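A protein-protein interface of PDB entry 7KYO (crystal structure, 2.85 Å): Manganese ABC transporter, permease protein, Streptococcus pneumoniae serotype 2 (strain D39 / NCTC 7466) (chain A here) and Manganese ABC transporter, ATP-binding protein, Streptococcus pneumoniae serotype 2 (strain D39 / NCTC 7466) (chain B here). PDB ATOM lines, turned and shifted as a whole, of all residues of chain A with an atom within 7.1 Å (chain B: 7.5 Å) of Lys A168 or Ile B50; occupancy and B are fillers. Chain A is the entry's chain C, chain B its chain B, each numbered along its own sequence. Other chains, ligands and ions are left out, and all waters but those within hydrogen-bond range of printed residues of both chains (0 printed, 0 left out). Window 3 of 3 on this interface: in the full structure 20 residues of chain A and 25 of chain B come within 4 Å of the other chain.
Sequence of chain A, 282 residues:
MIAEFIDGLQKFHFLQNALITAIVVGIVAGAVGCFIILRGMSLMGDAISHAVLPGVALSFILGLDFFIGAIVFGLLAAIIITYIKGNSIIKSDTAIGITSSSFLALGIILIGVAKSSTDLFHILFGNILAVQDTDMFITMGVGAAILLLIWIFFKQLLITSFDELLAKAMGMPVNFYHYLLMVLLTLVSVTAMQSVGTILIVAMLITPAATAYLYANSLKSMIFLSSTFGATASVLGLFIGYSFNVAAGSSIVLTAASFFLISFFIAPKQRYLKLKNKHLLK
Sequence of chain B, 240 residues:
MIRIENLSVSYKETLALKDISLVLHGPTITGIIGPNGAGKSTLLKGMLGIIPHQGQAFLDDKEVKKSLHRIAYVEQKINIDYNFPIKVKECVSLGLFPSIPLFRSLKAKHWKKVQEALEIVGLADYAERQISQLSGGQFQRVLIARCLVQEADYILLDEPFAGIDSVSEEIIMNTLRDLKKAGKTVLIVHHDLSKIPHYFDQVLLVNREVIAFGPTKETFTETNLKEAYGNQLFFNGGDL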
ATOM      1  N   THR A 160     -31.651  27.418  -1.840  1.00  0.00           N
ATOM      2  CA  THR A 160     -30.410  28.017  -2.346  1.00  0.00           C
ATOM      3  C   THR A 160     -30.090  29.362  -1.677  1.00  0.00           C
ATOM      4  O   THR A 160     -28.926  29.762  -1.628  1.00  0.00           O
ATOM      5  CB  THR A 160     -30.447  28.216  -3.876  1.00  0.00           C
ATOM      6  OG1 THR A 160     -31.576  29.021  -4.234  1.00  0.00           O
ATOM      7  CG2 THR A 160     -30.521  26.874  -4.602  1.00  0.00           C
ATOM      8  N   ASP A 163     -29.575  27.858   2.561  1.00  0.00           N
ATOM      9  CA  ASP A 163     -28.525  26.864   2.779  1.00  0.00           C
ATOM     10  C   ASP A 163     -27.964  26.358   1.450  1.00  0.00           C
ATOM     11  O   ASP A 163     -28.323  25.279   0.967  1.00  0.00           O
ATOM     12  CB  ASP A 163     -29.070  25.715   3.635  1.00  0.00           C
ATOM     13  CG  ASP A 163     -27.976  24.828   4.195  1.00  0.00           C
ATOM     14  OD1 ASP A 163     -26.952  24.634   3.511  1.00  0.00           O
ATOM     15  OD2 ASP A 163     -28.141  24.320   5.324  1.00  0.00           O
ATOM     16  N   GLU A 164     -27.064  27.156   0.882  1.00  0.00           N
ATOM     17  CA  GLU A 164     -26.432  26.863  -0.405  1.00  0.00           C
ATOM     18  C   GLU A 164     -25.604  25.574  -0.395  1.00  0.00           C
ATOM     19  O   GLU A 164     -25.580  24.841  -1.381  1.00  0.00           O
ATOM     20  CB  GLU A 164     -25.554  28.047  -0.825  1.00  0.00           C
ATOM     21  CG  GLU A 164     -24.874  27.882  -2.175  1.00  0.00           C
ATOM     22  CD  GLU A 164     -24.647  29.202  -2.895  1.00  0.00           C
ATOM     23  OE1 GLU A 164     -23.474  29.511  -3.207  1.00  0.00           O
ATOM     24  OE2 GLU A 164     -25.643  29.926  -3.152  1.00  0.00           O
ATOM     25  N   LEU A 165     -24.941  25.304   0.724  1.00  0.00           N
ATOM     26  CA  LEU A 165     -24.057  24.142   0.850  1.00  0.00           C
ATOM     27  C   LEU A 165     -24.837  22.820   0.843  1.00  0.00           C
ATOM     28  O   LEU A 165     -24.354  21.815   0.320  1.00  0.00           O
ATOM     29  CB  LEU A 165     -23.209  24.264   2.123  1.00  0.00           C
ATOM     30  CG  LEU A 165     -21.824  23.624   2.115  1.00  0.00           C
ATOM     31  CD1 LEU A 165     -20.933  24.227   1.036  1.00  0.00           C
ATOM     32  CD2 LEU A 165     -21.194  23.798   3.488  1.00  0.00           C
ATOM     33  N   LEU A 166     -26.037  22.832   1.425  1.00  0.00           N
ATOM     34  CA  LEU A 166     -26.946  21.685   1.378  1.00  0.00           C
ATOM     35  C   LEU A 166     -27.455  21.455  -0.045  1.00  0.00           C
ATOM     36  O   LEU A 166     -27.466  20.318  -0.518  1.00  0.00           O
ATOM     37  CB  LEU A 166     -28.131  21.892   2.329  1.00  0.00           C
ATOM     38  CG  LEU A 166     -29.157  20.759   2.485  1.00  0.00           C
ATOM     39  CD1 LEU A 166     -28.521  19.508   3.078  1.00  0.00           C
ATOM     40  CD2 LEU A 166     -30.341  21.224   3.326  1.00  0.00           C
ATOM     41  N   ALA A 167     -27.867  22.535  -0.714  1.00  0.00           N
ATOM     42  CA  ALA A 167     -28.339  22.477  -2.108  1.00  0.00           C
ATOM     43  C   ALA A 167     -27.308  21.847  -3.049  1.00  0.00           C
ATOM     44  O   ALA A 167     -27.666  21.050  -3.917  1.00  0.00           O
ATOM     45  CB  ALA A 167     -28.717  23.867  -2.597  1.00  0.00           C
ATOM     46  N   LYS A 168     -26.038  22.203  -2.862  1.00  0.00           N
ATOM     47  CA  LYS A 168     -24.931  21.569  -3.585  1.00  0.00           C
ATOM     48  C   LYS A 168     -24.785  20.080  -3.233  1.00  0.00           C
ATOM     49  O   LYS A 168     -24.597  19.247  -4.124  1.00  0.00           O
ATOM     50  CB  LYS A 168     -23.613  22.302  -3.312  1.00  0.00           C
ATOM     51  CG  LYS A 168     -23.550  23.702  -3.901  1.00  0.00           C
ATOM     52  CD  LYS A 168     -22.204  24.355  -3.630  1.00  0.00           C
ATOM     53  CE  LYS A 168     -22.163  25.795  -4.117  1.00  0.00           C
ATOM     54  NZ  LYS A 168     -20.925  26.486  -3.659  1.00  0.00           N
ATOM     55  N   ALA A 169     -24.890  19.754  -1.943  1.00  0.00           N
ATOM     56  CA  ALA A 169     -24.843  18.356  -1.472  1.00  0.00           C
ATOM     57  C   ALA A 169     -25.999  17.465  -1.970  1.00  0.00           C
ATOM     58  O   ALA A 169     -25.860  16.241  -2.003  1.00  0.00           O
ATOM     59  CB  ALA A 169     -24.772  18.315   0.047  1.00  0.00           C
ATOM     60  N   MET A 170     -27.128  18.075  -2.340  1.00  0.00           N
ATOM     61  CA  MET A 170     -28.269  17.358  -2.940  1.00  0.00           C
ATOM     62  C   MET A 170     -28.244  17.347  -4.482  1.00  0.00           C
ATOM     63  O   MET A 170     -29.165  16.822  -5.115  1.00  0.00           O
ATOM     64  CB  MET A 170     -29.586  17.959  -2.433  1.00  0.00           C
ATOM     65  CG  MET A 170     -29.740  17.869  -0.918  1.00  0.00           C
ATOM     66  SD  MET A 170     -31.318  18.393  -0.205  1.00  0.00           S
ATOM     67  CE  MET A 170     -31.727  19.828  -1.191  1.00  0.00           C
ATOM     68  N   GLY A 171     -27.195  17.918  -5.077  1.00  0.00           N
ATOM     69  CA  GLY A 171     -27.001  17.902  -6.523  1.00  0.00           C
ATOM     70  C   GLY A 171     -27.886  18.868  -7.285  1.00  0.00           C
ATOM     71  O   GLY A 171     -28.298  18.565  -8.402  1.00  0.00           O
ATOM     72  N   MET A 172     -28.169  20.029  -6.694  1.00  0.00           N
ATOM     73  CA  MET A 172     -28.997  21.050  -7.346  1.00  0.00           C
ATOM     74  C   MET A 172     -28.121  21.985  -8.177  1.00  0.00           C
ATOM     75  O   MET A 172     -26.997  22.295  -7.773  1.00  0.00           O
ATOM     76  CB  MET A 172     -29.781  21.870  -6.316  1.00  0.00           C
ATOM     77  CG  MET A 172     -30.838  21.078  -5.557  1.00  0.00           C
ATOM     78  SD  MET A 172     -31.700  22.057  -4.308  1.00  0.00           S
ATOM     79  CE  MET A 172     -32.512  23.294  -5.318  1.00  0.00           C
ATOM     80  N   PRO A 173     -28.633  22.444  -9.341  1.00  0.00           N
ATOM     81  CA  PRO A 173     -27.897  23.427 -10.135  1.00  0.00           C
ATOM     82  C   PRO A 173     -28.001  24.811  -9.487  1.00  0.00           C
ATOM     83  O   PRO A 173     -28.904  25.591  -9.803  1.00  0.00           O
ATOM     84  CB  PRO A 173     -28.598  23.366 -11.497  1.00  0.00           C
ATOM     85  CG  PRO A 173     -30.001  22.993 -11.172  1.00  0.00           C
ATOM     86  CD  PRO A 173     -29.942  22.123  -9.946  1.00  0.00           C
ATOM     87  N   VAL A 174     -27.078  25.093  -8.570  1.00  0.00           N
ATOM     88  CA  VAL A 174     -27.123  26.318  -7.768  1.00  0.00           C
ATOM     89  C   VAL A 174     -26.920  27.572  -8.621  1.00  0.00           C
ATOM     90  O   VAL A 174     -27.588  28.584  -8.398  1.00  0.00           O
ATOM     91  CB  VAL A 174     -26.097  26.271  -6.610  1.00  0.00           C
ATOM     92  CG1 VAL A 174     -26.003  27.615  -5.888  1.00  0.00           C
ATOM     93  CG2 VAL A 174     -26.470  25.164  -5.627  1.00  0.00           C
ATOM     94  N   ASN A 175     -26.011  27.499  -9.593  1.00  0.00           N
ATOM     95  CA  ASN A 175     -25.724  28.640 -10.474  1.00  0.00           C
ATOM     96  C   ASN A 175     -26.877  29.015 -11.405  1.00  0.00           C
ATOM     97  O   ASN A 175     -26.996  30.179 -11.780  1.00  0.00           O
ATOM     98  CB  ASN A 175     -24.446  28.399 -11.286  1.00  0.00           C
ATOM     99  CG  ASN A 175     -23.196  28.404 -10.423  1.00  0.00           C
ATOM    100  OD1 ASN A 175     -23.034  29.252  -9.539  1.00  0.00           O
ATOM    101  ND2 ASN A 175     -22.299  27.458 -10.677  1.00  0.00           N
ATOM    102  N   HIS A 178     -28.749  31.454  -9.312  1.00  0.00           N
ATOM    103  CA  HIS A 178     -28.007  32.731  -9.274  1.00  0.00           C
ATOM    104  C   HIS A 178     -28.330  33.571 -10.508  1.00  0.00           C
ATOM    105  O   HIS A 178     -28.663  34.751 -10.390  1.00  0.00           O
ATOM    106  CB  HIS A 178     -26.482  32.521  -9.205  1.00  0.00           C
ATOM    107  CG  HIS A 178     -25.966  32.194  -7.836  1.00  0.00           C
ATOM    108  ND1 HIS A 178     -26.236  32.971  -6.729  1.00  0.00           N
ATOM    109  CD2 HIS A 178     -25.164  31.189  -7.403  1.00  0.00           C
ATOM    110  CE1 HIS A 178     -25.643  32.447  -5.670  1.00  0.00           C
ATOM    111  NE2 HIS A 178     -24.986  31.366  -6.052  1.00  0.00           N
ATOM    112  N   LEU B  44     -14.880  15.522   3.090  1.00  0.00           N
ATOM    113  CA  LEU B  44     -16.324  15.324   2.904  1.00  0.00           C
ATOM    114  C   LEU B  44     -16.853  16.112   1.703  1.00  0.00           C
ATOM    115  O   LEU B  44     -17.694  15.613   0.954  1.00  0.00           O
ATOM    116  CB  LEU B  44     -17.107  15.722   4.161  1.00  0.00           C
ATOM    117  CG  LEU B  44     -16.831  14.986   5.478  1.00  0.00           C
ATOM    118  CD1 LEU B  44     -17.881  15.375   6.511  1.00  0.00           C
ATOM    119  CD2 LEU B  44     -16.787  13.474   5.296  1.00  0.00           C
ATOM    120  N   LYS B  45     -16.356  17.338   1.533  1.00  0.00           N
ATOM    121  CA  LYS B  45     -16.743  18.198   0.407  1.00  0.00           C
ATOM    122  C   LYS B  45     -16.179  17.705  -0.928  1.00  0.00           C
ATOM    123  O   LYS B  45     -16.814  17.876  -1.967  1.00  0.00           O
ATOM    124  CB  LYS B  45     -16.322  19.647   0.667  1.00  0.00           C
ATOM    125  CG  LYS B  45     -17.044  20.272   1.849  1.00  0.00           C
ATOM    126  CD  LYS B  45     -16.641  21.719   2.074  1.00  0.00           C
ATOM    127  CE  LYS B  45     -17.371  22.299   3.277  1.00  0.00           C
ATOM    128  NZ  LYS B  45     -17.208  23.775   3.396  1.00  0.00           N
ATOM    129  N   GLY B  46     -14.990  17.104  -0.893  1.00  0.00           N
ATOM    130  CA  GLY B  46     -14.399  16.451  -2.062  1.00  0.00           C
ATOM    131  C   GLY B  46     -15.137  15.186  -2.477  1.00  0.00           C
ATOM    132  O   GLY B  46     -15.295  14.921  -3.672  1.00  0.00           O
ATOM    133  N   MET B  47     -15.577  14.405  -1.489  1.00  0.00           N
ATOM    134  CA  MET B  47     -16.411  13.223  -1.734  1.00  0.00           C
ATOM    135  C   MET B  47     -17.715  13.557  -2.446  1.00  0.00           C
ATOM    136  O   MET B  47     -18.091  12.873  -3.381  1.00  0.00           O
ATOM    137  CB  MET B  47     -16.759  12.514  -0.428  1.00  0.00           C
ATOM    138  CG  MET B  47     -15.644  11.664   0.137  1.00  0.00           C
ATOM    139  SD  MET B  47     -16.062  11.088   1.786  1.00  0.00           S
ATOM    140  CE  MET B  47     -17.483  10.059   1.416  1.00  0.00           C
ATOM    141  N   LEU B  48     -18.399  14.600  -1.989  1.00  0.00           N
ATOM    142  CA  LEU B  48     -19.688  14.988  -2.568  1.00  0.00           C
ATOM    143  C   LEU B  48     -19.577  15.712  -3.916  1.00  0.00           C
ATOM    144  O   LEU B  48     -20.562  15.792  -4.651  1.00  0.00           O
ATOM    145  CB  LEU B  48     -20.477  15.845  -1.569  1.00  0.00           C
ATOM    146  CG  LEU B  48     -20.850  15.127  -0.266  1.00  0.00           C
ATOM    147  CD1 LEU B  48     -21.338  16.120   0.776  1.00  0.00           C
ATOM    148  CD2 LEU B  48     -21.889  14.038  -0.510  1.00  0.00           C
ATOM    149  N   GLY B  49     -18.389  16.223  -4.241  1.00  0.00           N
ATOM    150  CA  GLY B  49     -18.178  16.994  -5.463  1.00  0.00           C
ATOM    151  C   GLY B  49     -18.734  18.404  -5.366  1.00  0.00           C
ATOM    152  O   GLY B  49     -19.098  18.996  -6.381  1.00  0.00           O
ATOM    153  N   ILE B  50     -18.789  18.935  -4.142  1.00  0.00           N
ATOM    154  CA  ILE B  50     -19.244  20.304  -3.875  1.00  0.00           C
ATOM    155  C   ILE B  50     -18.167  21.289  -4.320  1.00  0.00           C
ATOM    156  O   ILE B  50     -18.450  22.241  -5.045  1.00  0.00           O
ATOM    157  CB  ILE B  50     -19.550  20.515  -2.369  1.00  0.00           C
ATOM    158  CG1 ILE B  50     -20.748  19.656  -1.948  1.00  0.00           C
ATOM    159  CG2 ILE B  50     -19.809  21.990  -2.054  1.00  0.00           C
ATOM    160  CD1 ILE B  50     -20.935  19.547  -0.449  1.00  0.00           C
ATOM    161  N   ILE B  51     -16.945  21.055  -3.843  1.00  0.00           N
ATOM    162  CA  ILE B  51     -15.754  21.798  -4.271  1.00  0.00           C
ATOM    163  C   ILE B  51     -15.058  21.057  -5.424  1.00  0.00           C
ATOM    164  O   ILE B  51     -15.289  19.858  -5.607  1.00  0.00           O
ATOM    165  CB  ILE B  51     -14.768  22.039  -3.097  1.00  0.00           C
ATOM    166  CG1 ILE B  51     -14.108  20.726  -2.616  1.00  0.00           C
ATOM    167  CG2 ILE B  51     -15.479  22.765  -1.960  1.00  0.00           C
ATOM    168  CD1 ILE B  51     -13.310  20.852  -1.336  1.00  0.00           C
ATOM    169  N   PRO B  52     -14.205  21.762  -6.203  1.00  0.00           N
ATOM    170  CA  PRO B  52     -13.458  21.063  -7.255  1.00  0.00           C
ATOM    171  C   PRO B  52     -12.425  20.089  -6.679  1.00  0.00           C
ATOM    172  O   PRO B  52     -11.775  20.403  -5.678  1.00  0.00           O
ATOM    173  CB  PRO B  52     -12.764  22.201  -8.023  1.00  0.00           C
ATOM    174  CG  PRO B  52     -13.467  23.450  -7.615  1.00  0.00           C
ATOM    175  CD  PRO B  52     -13.923  23.208  -6.213  1.00  0.00           C
ATOM    176  N   HIS B  53     -12.294  18.923  -7.313  1.00  0.00           N
ATOM    177  CA  HIS B  53     -11.389  17.859  -6.860  1.00  0.00           C
ATOM    178  C   HIS B  53     -10.786  17.109  -8.049  1.00  0.00           C
ATOM    179  O   HIS B  53     -11.264  17.239  -9.177  1.00  0.00           O
ATOM    180  CB  HIS B  53     -12.136  16.883  -5.944  1.00  0.00           C
ATOM    181  CG  HIS B  53     -13.309  16.220  -6.597  1.00  0.00           C
ATOM    182  ND1 HIS B  53     -13.265  14.925  -7.065  1.00  0.00           N
ATOM    183  CD2 HIS B  53     -14.552  16.678  -6.875  1.00  0.00           C
ATOM    184  CE1 HIS B  53     -14.432  14.612  -7.600  1.00  0.00           C
ATOM    185  NE2 HIS B  53     -15.231  15.658  -7.496  1.00  0.00           N
ATOM    186  N   LEU B  68     -26.265  11.077  -5.390  1.00  0.00           N
ATOM    187  CA  LEU B  68     -26.351  11.962  -4.215  1.00  0.00           C
ATOM    188  C   LEU B  68     -27.614  11.751  -3.367  1.00  0.00           C
ATOM    189  O   LEU B  68     -27.629  12.109  -2.194  1.00  0.00           O
ATOM    190  CB  LEU B  68     -26.245  13.437  -4.626  1.00  0.00           C
ATOM    191  CG  LEU B  68     -24.871  13.895  -5.131  1.00  0.00           C
ATOM    192  CD1 LEU B  68     -24.980  15.224  -5.863  1.00  0.00           C
ATOM    193  CD2 LEU B  68     -23.862  13.992  -3.991  1.00  0.00           C
ATOM    194  N   TYR B  73     -25.701  15.266   3.906  1.00  0.00           N
ATOM    195  CA  TYR B  73     -24.583  16.074   4.394  1.00  0.00           C
ATOM    196  C   TYR B  73     -25.084  17.049   5.449  1.00  0.00           C
ATOM    197  O   TYR B  73     -25.896  17.925   5.145  1.00  0.00           O
ATOM    198  CB  TYR B  73     -23.942  16.843   3.233  1.00  0.00           C
ATOM    199  CG  TYR B  73     -22.751  17.707   3.618  1.00  0.00           C
ATOM    200  CD1 TYR B  73     -21.644  17.159   4.267  1.00  0.00           C
ATOM    201  CD2 TYR B  73     -22.720  19.071   3.310  1.00  0.00           C
ATOM    202  CE1 TYR B  73     -20.551  17.942   4.609  1.00  0.00           C
ATOM    203  CE2 TYR B  73     -21.628  19.862   3.648  1.00  0.00           C
ATOM    204  CZ  TYR B  73     -20.547  19.296   4.298  1.00  0.00           C
ATOM    205  OH  TYR B  73     -19.459  20.075   4.642  1.00  0.00           O
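Hydrophobic or aromatic side chains of chain A within 4 Å of the printed part of chain B: Leu A165, Leu A166 and Ala A169.
Of the 12 printed residues of chain B, 4 touch a printed residue of chain A.
Hydrophobic or aromatic side chains of chain B within 4 Å of the printed part of chain A: Ile B50, Leu B68 and Tyr B73.
Among the printed residues, 8 pairs touch across the chains.
No residue of chain B comes within 4 Å of Ala A167.
No residue of chain A comes within 4 Å of Gly B49.
Printed residues of chain A within 4 Å of Leu B68: Ala A169 (3.6 Å) and Gly A171 (3.4 Å).
Of the printed residues of chain B, Leu A165 touches Lys B45 (3.99 Å), Ile B50 (3.98 Å) and Tyr B73 (3.96 Å).
Of the printed residues of chain B, Gly A171 touches Leu B68 (3.4 Å).
Of the printed residues of chain B, Leu A166 touches Tyr B73.
Met A172 touches none of the printed residues of chain B.
The nearest printed residue of chain B that does not touch Leu A166 is Ile B50 (6.4 Å).
The backbone carbonyl oxygen of Lys B45 lies within hydrogen-bond range of the backbone NH of Ile B50 (3.1 Å).
N of Leu A166 is in hydrogen-bond range of OD1 of Asp A163, 2.9 Å away.
OE1 of Glu A164 lies within salt-bridge range of NZ of Lys A168 (3.98 Å).
Among the printed residues, pairs that only touch across the chains: Leu A165 with Lys B45 (3.99 Å), Leu A165 with Ile B50 (3.98 Å), Leu A165 with Tyr B73 (3.96 Å), Leu A166 with Tyr B73 (3.7 Å), Lys A168 with Ile B50 (3.7 Å), Ala A169 with Leu B68 (3.6 Å), Ala A169 with Tyr B73 (3.6 Å) and Gly A171 with Leu B68 (3.4 Å).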
